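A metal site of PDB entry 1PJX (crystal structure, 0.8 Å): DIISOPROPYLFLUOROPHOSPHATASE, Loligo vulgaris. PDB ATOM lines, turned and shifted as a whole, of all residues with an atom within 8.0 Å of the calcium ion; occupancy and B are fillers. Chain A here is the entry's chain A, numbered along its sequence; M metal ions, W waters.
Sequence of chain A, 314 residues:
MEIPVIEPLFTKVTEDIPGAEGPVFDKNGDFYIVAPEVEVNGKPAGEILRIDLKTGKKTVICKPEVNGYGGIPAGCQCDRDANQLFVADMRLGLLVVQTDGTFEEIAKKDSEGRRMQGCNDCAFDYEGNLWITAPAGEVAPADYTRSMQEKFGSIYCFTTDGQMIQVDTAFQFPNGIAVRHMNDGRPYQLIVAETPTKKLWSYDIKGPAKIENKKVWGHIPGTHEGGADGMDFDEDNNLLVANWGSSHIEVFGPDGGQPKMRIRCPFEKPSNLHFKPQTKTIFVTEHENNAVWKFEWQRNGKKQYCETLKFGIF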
ATOM      1  N   GLU A  21     -35.246  20.576  28.130  1.00  0.00           N
ATOM      2  CA  GLU A  21     -34.614  21.558  27.253  1.00  0.00           C
ATOM      3  C   GLU A  21     -33.488  22.244  27.969  1.00  0.00           C
ATOM      4  O   GLU A  21     -33.237  22.079  29.182  1.00  0.00           O
ATOM      5  CB  GLU A  21     -35.653  22.585  26.744  1.00  0.00           C
ATOM      6  CG  GLU A  21     -36.110  22.381  25.306  1.00  0.00           C
ATOM      7  CD  GLU A  21     -35.151  22.919  24.294  1.00  0.00           C
ATOM      8  OE1 GLU A  21     -33.913  23.011  24.597  1.00  0.00           O
ATOM      9  OE2 GLU A  21     -35.640  23.274  23.198  1.00  0.00           O
ATOM     10  N   GLY A  22     -32.765  23.074  27.207  1.00  0.00           N
ATOM     11  CA  GLY A  22     -31.814  24.003  27.709  1.00  0.00           C
ATOM     12  C   GLY A  22     -30.807  23.487  28.740  1.00  0.00           C
ATOM     13  O   GLY A  22     -30.562  24.150  29.744  1.00  0.00           O
ATOM     14  N   PRO A  23     -30.166  22.339  28.473  1.00  0.00           N
ATOM     15  CA  PRO A  23     -29.146  21.873  29.419  1.00  0.00           C
ATOM     16  C   PRO A  23     -28.030  22.861  29.497  1.00  0.00           C
ATOM     17  O   PRO A  23     -27.536  23.410  28.484  1.00  0.00           O
ATOM     18  CB  PRO A  23     -28.708  20.531  28.791  1.00  0.00           C
ATOM     19  CG  PRO A  23     -28.967  20.702  27.302  1.00  0.00           C
ATOM     20  CD  PRO A  23     -30.233  21.543  27.244  1.00  0.00           C
ATOM     21  N   VAL A  24     -27.501  23.086  30.715  1.00  0.00           N
ATOM     22  CA  VAL A  24     -26.470  24.074  30.891  1.00  0.00           C
ATOM     23  C   VAL A  24     -25.696  23.777  32.176  1.00  0.00           C
ATOM     24  O   VAL A  24     -26.269  23.298  33.150  1.00  0.00           O
ATOM     25  CB  VAL A  24     -27.066  25.509  30.897  1.00  0.00           C
ATOM     26  CG1 VAL A  24     -28.024  25.727  32.092  1.00  0.00           C
ATOM     27  CG2 VAL A  24     -26.038  26.589  30.795  1.00  0.00           C
ATOM     28  N   PHE A  25     -24.410  24.087  32.160  1.00  0.00           N
ATOM     29  CA  PHE A  25     -23.565  24.081  33.363  1.00  0.00           C
ATOM     30  C   PHE A  25     -23.307  25.496  33.786  1.00  0.00           C
ATOM     31  O   PHE A  25     -23.048  26.382  32.945  1.00  0.00           O
ATOM     32  CB  PHE A  25     -22.248  23.341  33.123  1.00  0.00           C
ATOM     33  CG  PHE A  25     -22.420  21.837  33.094  1.00  0.00           C
ATOM     34  CD1 PHE A  25     -22.651  21.152  31.908  1.00  0.00           C
ATOM     35  CD2 PHE A  25     -22.372  21.086  34.257  1.00  0.00           C
ATOM     36  CE1 PHE A  25     -22.826  19.804  31.904  1.00  0.00           C
ATOM     37  CE2 PHE A  25     -22.528  19.736  34.216  1.00  0.00           C
ATOM     38  CZ  PHE A  25     -22.769  19.068  33.049  1.00  0.00           C
ATOM     39  N   CYS A  76     -30.971  28.010  27.591  1.00  0.00           N
ATOM     40  CA  CYS A  76     -30.149  28.658  28.585  1.00  0.00           C
ATOM     41  C   CYS A  76     -28.734  28.900  28.117  1.00  0.00           C
ATOM     42  O   CYS A  76     -28.149  28.108  27.353  1.00  0.00           O
ATOM     43  CB  CYS A  76     -30.022  27.794  29.853  1.00  0.00           C
ATOM     44  SG  CYS A  76     -31.584  27.294  30.608  1.00  0.00           S
ATOM     45  N   GLN A  77     -28.119  29.945  28.702  1.00  0.00           N
ATOM     46  CA  GLN A  77     -26.694  30.164  28.683  1.00  0.00           C
ATOM     47  C   GLN A  77     -26.270  30.665  30.061  1.00  0.00           C
ATOM     48  O   GLN A  77     -27.012  31.439  30.683  1.00  0.00           O
ATOM     49  CB  GLN A  77     -26.277  31.236  27.664  1.00  0.00           C
ATOM     50  CG  GLN A  77     -26.464  30.850  26.207  1.00  0.00           C
ATOM     51  CD  GLN A  77     -25.358  29.930  25.718  1.00  0.00           C
ATOM     52  OE1 GLN A  77     -24.346  30.354  25.195  1.00  0.00           O
ATOM     53  NE2 GLN A  77     -25.564  28.639  25.928  1.00  0.00           N
ATOM     54  N   ASP A 121     -33.970  29.712  22.262  1.00  0.00           N
ATOM     55  CA  ASP A 121     -32.602  29.371  22.629  1.00  0.00           C
ATOM     56  C   ASP A 121     -31.729  30.591  22.481  1.00  0.00           C
ATOM     57  O   ASP A 121     -32.125  31.626  21.914  1.00  0.00           O
ATOM     58  CB  ASP A 121     -32.092  28.143  21.841  1.00  0.00           C
ATOM     59  CG  ASP A 121     -31.086  27.287  22.595  1.00  0.00           C
ATOM     60  OD1 ASP A 121     -30.614  27.697  23.688  1.00  0.00           O
ATOM     61  OD2 ASP A 121     -30.767  26.176  22.070  1.00  0.00           O
ATOM     62  N   CYS A 122     -30.507  30.491  23.008  1.00  0.00           N
ATOM     63  CA  CYS A 122     -29.593  31.615  22.971  1.00  0.00           C
ATOM     64  C   CYS A 122     -28.145  31.112  23.011  1.00  0.00           C
ATOM     65  O   CYS A 122     -27.871  29.996  23.467  1.00  0.00           O
ATOM     66  CB  CYS A 122     -29.921  32.674  24.031  1.00  0.00           C
ATOM     67  SG  CYS A 122     -29.862  32.090  25.742  1.00  0.00           S
ATOM     68  N   ILE A 177     -29.112  27.849  18.054  1.00  0.00           N
ATOM     69  CA  ILE A 177     -28.260  28.954  17.627  1.00  0.00           C
ATOM     70  C   ILE A 177     -26.885  28.714  18.209  1.00  0.00           C
ATOM     71  O   ILE A 177     -26.761  28.182  19.324  1.00  0.00           O
ATOM     72  CB  ILE A 177     -28.909  30.295  18.033  1.00  0.00           C
ATOM     73  CG1 ILE A 177     -28.173  31.513  17.462  1.00  0.00           C
ATOM     74  CG2 ILE A 177     -29.154  30.407  19.529  1.00  0.00           C
ATOM     75  CD1 ILE A 177     -29.059  32.766  17.450  1.00  0.00           C
ATOM     76  N   GLY A 230     -31.555  21.939  19.074  1.00  0.00           N
ATOM     77  CA  GLY A 230     -30.420  22.556  19.703  1.00  0.00           C
ATOM     78  C   GLY A 230     -29.089  22.203  19.094  1.00  0.00           C
ATOM     79  O   GLY A 230     -28.939  21.166  18.432  1.00  0.00           O
ATOM     80  N   MET A 231     -28.081  23.011  19.360  1.00  0.00           N
ATOM     81  CA  MET A 231     -26.774  22.819  18.761  1.00  0.00           C
ATOM     82  C   MET A 231     -25.658  23.327  19.652  1.00  0.00           C
ATOM     83  O   MET A 231     -25.855  24.226  20.496  1.00  0.00           O
ATOM     84  CB  MET A 231     -26.685  23.516  17.393  1.00  0.00           C
ATOM     85  CG  MET A 231     -26.829  24.985  17.494  1.00  0.00           C
ATOM     86  SD  MET A 231     -26.733  25.872  15.900  1.00  0.00           S
ATOM     87  CE  MET A 231     -28.063  25.036  15.063  1.00  0.00           C
ATOM     88  N   ASP A 232     -24.454  22.823  19.424  1.00  0.00           N
ATOM     89  CA  ASP A 232     -23.247  23.349  20.057  1.00  0.00           C
ATOM     90  C   ASP A 232     -22.036  22.898  19.254  1.00  0.00           C
ATOM     91  O   ASP A 232     -22.073  21.840  18.597  1.00  0.00           O
ATOM     92  CB  ASP A 232     -23.062  22.900  21.518  1.00  0.00           C
ATOM     93  CG  ASP A 232     -23.693  23.783  22.558  1.00  0.00           C
ATOM     94  OD1 ASP A 232     -23.540  25.031  22.467  1.00  0.00           O
ATOM     95  OD2 ASP A 232     -24.295  23.221  23.499  1.00  0.00           O
ATOM     96  N   PHE A 233     -20.970  23.657  19.373  1.00  0.00           N
ATOM     97  CA  PHE A 233     -19.701  23.304  18.752  1.00  0.00           C
ATOM     98  C   PHE A 233     -18.841  22.445  19.694  1.00  0.00           C
ATOM     99  O   PHE A 233     -18.788  22.657  20.897  1.00  0.00           O
ATOM    100  CB  PHE A 233     -18.885  24.593  18.458  1.00  0.00           C
ATOM    101  CG  PHE A 233     -19.399  25.345  17.262  1.00  0.00           C
ATOM    102  CD1 PHE A 233     -20.066  26.562  17.388  1.00  0.00           C
ATOM    103  CD2 PHE A 233     -19.214  24.825  15.982  1.00  0.00           C
ATOM    104  CE1 PHE A 233     -20.497  27.244  16.272  1.00  0.00           C
ATOM    105  CE2 PHE A 233     -19.666  25.532  14.874  1.00  0.00           C
ATOM    106  CZ  PHE A 233     -20.276  26.725  15.019  1.00  0.00           C
ATOM    107  N   LEU A 240     -22.591  20.088  16.372  1.00  0.00           N
ATOM    108  CA  LEU A 240     -23.476  18.985  16.702  1.00  0.00           C
ATOM    109  C   LEU A 240     -24.885  19.538  16.857  1.00  0.00           C
ATOM    110  O   LEU A 240     -25.086  20.535  17.567  1.00  0.00           O
ATOM    111  CB  LEU A 240     -23.027  18.251  17.969  1.00  0.00           C
ATOM    112  CG  LEU A 240     -21.696  17.502  17.833  1.00  0.00           C
ATOM    113  CD1 LEU A 240     -20.520  18.346  18.113  1.00  0.00           C
ATOM    114  CD2 LEU A 240     -21.664  16.293  18.665  1.00  0.00           C
ATOM    115  N   ASN A 272     -31.988  19.011  22.785  1.00  0.00           N
ATOM    116  CA  ASN A 272     -30.923  19.955  23.024  1.00  0.00           C
ATOM    117  C   ASN A 272     -29.757  19.251  23.698  1.00  0.00           C
ATOM    118  O   ASN A 272     -29.875  18.098  24.141  1.00  0.00           O
ATOM    119  CB  ASN A 272     -31.428  21.197  23.773  1.00  0.00           C
ATOM    120  CG  ASN A 272     -30.684  22.465  23.392  1.00  0.00           C
ATOM    121  OD1 ASN A 272     -29.567  22.426  22.895  1.00  0.00           O
ATOM    122  ND2 ASN A 272     -31.364  23.603  23.549  1.00  0.00           N
ATOM    123  N   LEU A 273     -28.616  19.912  23.720  1.00  0.00           N
ATOM    124  CA  LEU A 273     -27.399  19.255  24.133  1.00  0.00           C
ATOM    125  C   LEU A 273     -26.465  20.280  24.764  1.00  0.00           C
ATOM    126  O   LEU A 273     -26.580  21.493  24.570  1.00  0.00           O
ATOM    127  CB  LEU A 273     -26.794  18.440  23.003  1.00  0.00           C
ATOM    128  CG  LEU A 273     -26.512  19.190  21.705  1.00  0.00           C
ATOM    129  CD1 LEU A 273     -25.215  19.849  21.755  1.00  0.00           C
ATOM    130  CD2 LEU A 273     -26.421  18.226  20.448  1.00  0.00           C
ATOM    131  N   HIS A 274     -25.514  19.763  25.550  1.00  0.00           N
ATOM    132  CA  HIS A 274     -24.513  20.643  26.148  1.00  0.00           C
ATOM    133  C   HIS A 274     -23.329  19.805  26.589  1.00  0.00           C
ATOM    134  O   HIS A 274     -23.553  18.726  27.214  1.00  0.00           O
ATOM    135  CB  HIS A 274     -25.084  21.393  27.370  1.00  0.00           C
ATOM    136  CG  HIS A 274     -24.510  22.754  27.549  1.00  0.00           C
ATOM    137  ND1 HIS A 274     -24.833  23.762  26.626  1.00  0.00           N
ATOM    138  CD2 HIS A 274     -23.746  23.278  28.501  1.00  0.00           C
ATOM    139  CE1 HIS A 274     -24.234  24.858  27.101  1.00  0.00           C
ATOM    140  NE2 HIS A 274     -23.573  24.582  28.225  1.00  0.00           N
ATOM    141  N   PHE A 275     -22.119  20.274  26.381  1.00  0.00           N
ATOM    142  CA  PHE A 275     -20.947  19.608  26.918  1.00  0.00           C
ATOM    143  C   PHE A 275     -20.762  19.930  28.389  1.00  0.00           C
ATOM    144  O   PHE A 275     -20.984  21.055  28.842  1.00  0.00           O
ATOM    145  CB  PHE A 275     -19.677  20.041  26.176  1.00  0.00           C
ATOM    146  CG  PHE A 275     -19.517  19.464  24.794  1.00  0.00           C
ATOM    147  CD1 PHE A 275     -20.151  20.035  23.693  1.00  0.00           C
ATOM    148  CD2 PHE A 275     -18.702  18.362  24.604  1.00  0.00           C
ATOM    149  CE1 PHE A 275     -19.949  19.532  22.407  1.00  0.00           C
ATOM    150  CE2 PHE A 275     -18.495  17.861  23.339  1.00  0.00           C
ATOM    151  CZ  PHE A 275     -19.098  18.431  22.243  1.00  0.00           C
ATOM    152  N   ILE A 282     -21.345  14.829  26.493  1.00  0.00           N
ATOM    153  CA  ILE A 282     -22.478  15.590  26.034  1.00  0.00           C
ATOM    154  C   ILE A 282     -23.734  15.110  26.732  1.00  0.00           C
ATOM    155  O   ILE A 282     -24.090  13.924  26.670  1.00  0.00           O
ATOM    156  CB  ILE A 282     -22.659  15.482  24.512  1.00  0.00           C
ATOM    157  CG1 ILE A 282     -21.425  15.977  23.790  1.00  0.00           C
ATOM    158  CG2 ILE A 282     -23.892  16.273  24.068  1.00  0.00           C
ATOM    159  CD1 ILE A 282     -21.469  15.936  22.278  1.00  0.00           C
ATOM    160  N   PHE A 283     -24.418  16.040  27.390  1.00  0.00           N
ATOM    161  CA  PHE A 283     -25.728  15.831  27.971  1.00  0.00           C
ATOM    162  C   PHE A 283     -26.775  16.165  26.906  1.00  0.00           C
ATOM    163  O   PHE A 283     -26.659  17.209  26.238  1.00  0.00           O
ATOM    164  CB  PHE A 283     -25.888  16.688  29.216  1.00  0.00           C
ATOM    165  CG  PHE A 283     -25.071  16.188  30.357  1.00  0.00           C
ATOM    166  CD1 PHE A 283     -25.701  15.487  31.393  1.00  0.00           C
ATOM    167  CD2 PHE A 283     -23.677  16.321  30.416  1.00  0.00           C
ATOM    168  CE1 PHE A 283     -24.927  14.924  32.428  1.00  0.00           C
ATOM    169  CE2 PHE A 283     -22.941  15.787  31.438  1.00  0.00           C
ATOM    170  CZ  PHE A 283     -23.596  15.079  32.448  1.00  0.00           C
ATOM    171  N   GLN A 304     -17.741  27.483  26.371  1.00  0.00           N
ATOM    172  CA  GLN A 304     -18.772  28.485  26.421  1.00  0.00           C
ATOM    173  C   GLN A 304     -18.204  29.790  26.972  1.00  0.00           C
ATOM    174  O   GLN A 304     -17.144  29.822  27.604  1.00  0.00           O
ATOM    175  CB  GLN A 304     -19.894  27.970  27.304  1.00  0.00           C
ATOM    176  CG  GLN A 304     -20.657  26.759  26.717  1.00  0.00           C
ATOM    177  CD  GLN A 304     -21.792  27.194  25.860  1.00  0.00           C
ATOM    178  OE1 GLN A 304     -22.812  27.677  26.364  1.00  0.00           O
ATOM    179  NE2 GLN A 304     -21.720  27.017  24.571  1.00  0.00           N
HETATM  180 CA    CA M   1     -26.120  23.717  24.646  1.00  0.00          CA
HETATM  181  O   HOH W   1     -25.491  25.887  24.257  1.00  0.00           O
HETATM  182  O   HOH W   2     -27.418  24.022  22.829  1.00  0.00           O
HETATM  183  O   HOH W   3     -27.985  23.997  25.867  1.00  0.00           O
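N of Phe 283 is in hydrogen-bond range of O of His 274 (2.8 Å).
The side-chain amide nitrogen (NE2) of Gln 304 is in hydrogen-bond range of the side-chain carboxylate (OD1) of Asp 232 (3.4 Å).
A ring nitrogen (ND1) of His 274 lies close to the backbone carbonyl oxygen (O) of Pro 23 (3.3 Å).
The backbone NH (N) of Leu 240 sits at hydrogen-bond distance from the backbone carbonyl oxygen (O) of Asp 232.
The calcium ion is bound by the side-chain carboxylate of Asp 232 (2.2 Å), water W3 (2.2 Å), water W2 (2.3 Å), the backbone carbonyl oxygen of Leu 273 (2.3 Å), water W1 (2.3 Å) and a ring nitrogen (ND1) of His 274 (2.4 Å).
Water W1 lies within hydrogen-bond range of OD1 of Asp 232 (2.8 Å) and NE2 of Gln 77 (3.2 Å).
Water W2 bridges the side-chain amide oxygen (OD1) of Asn 272 (2.7 Å) and the backbone carbonyl oxygen (O) of Met 231 (2.8 Å).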
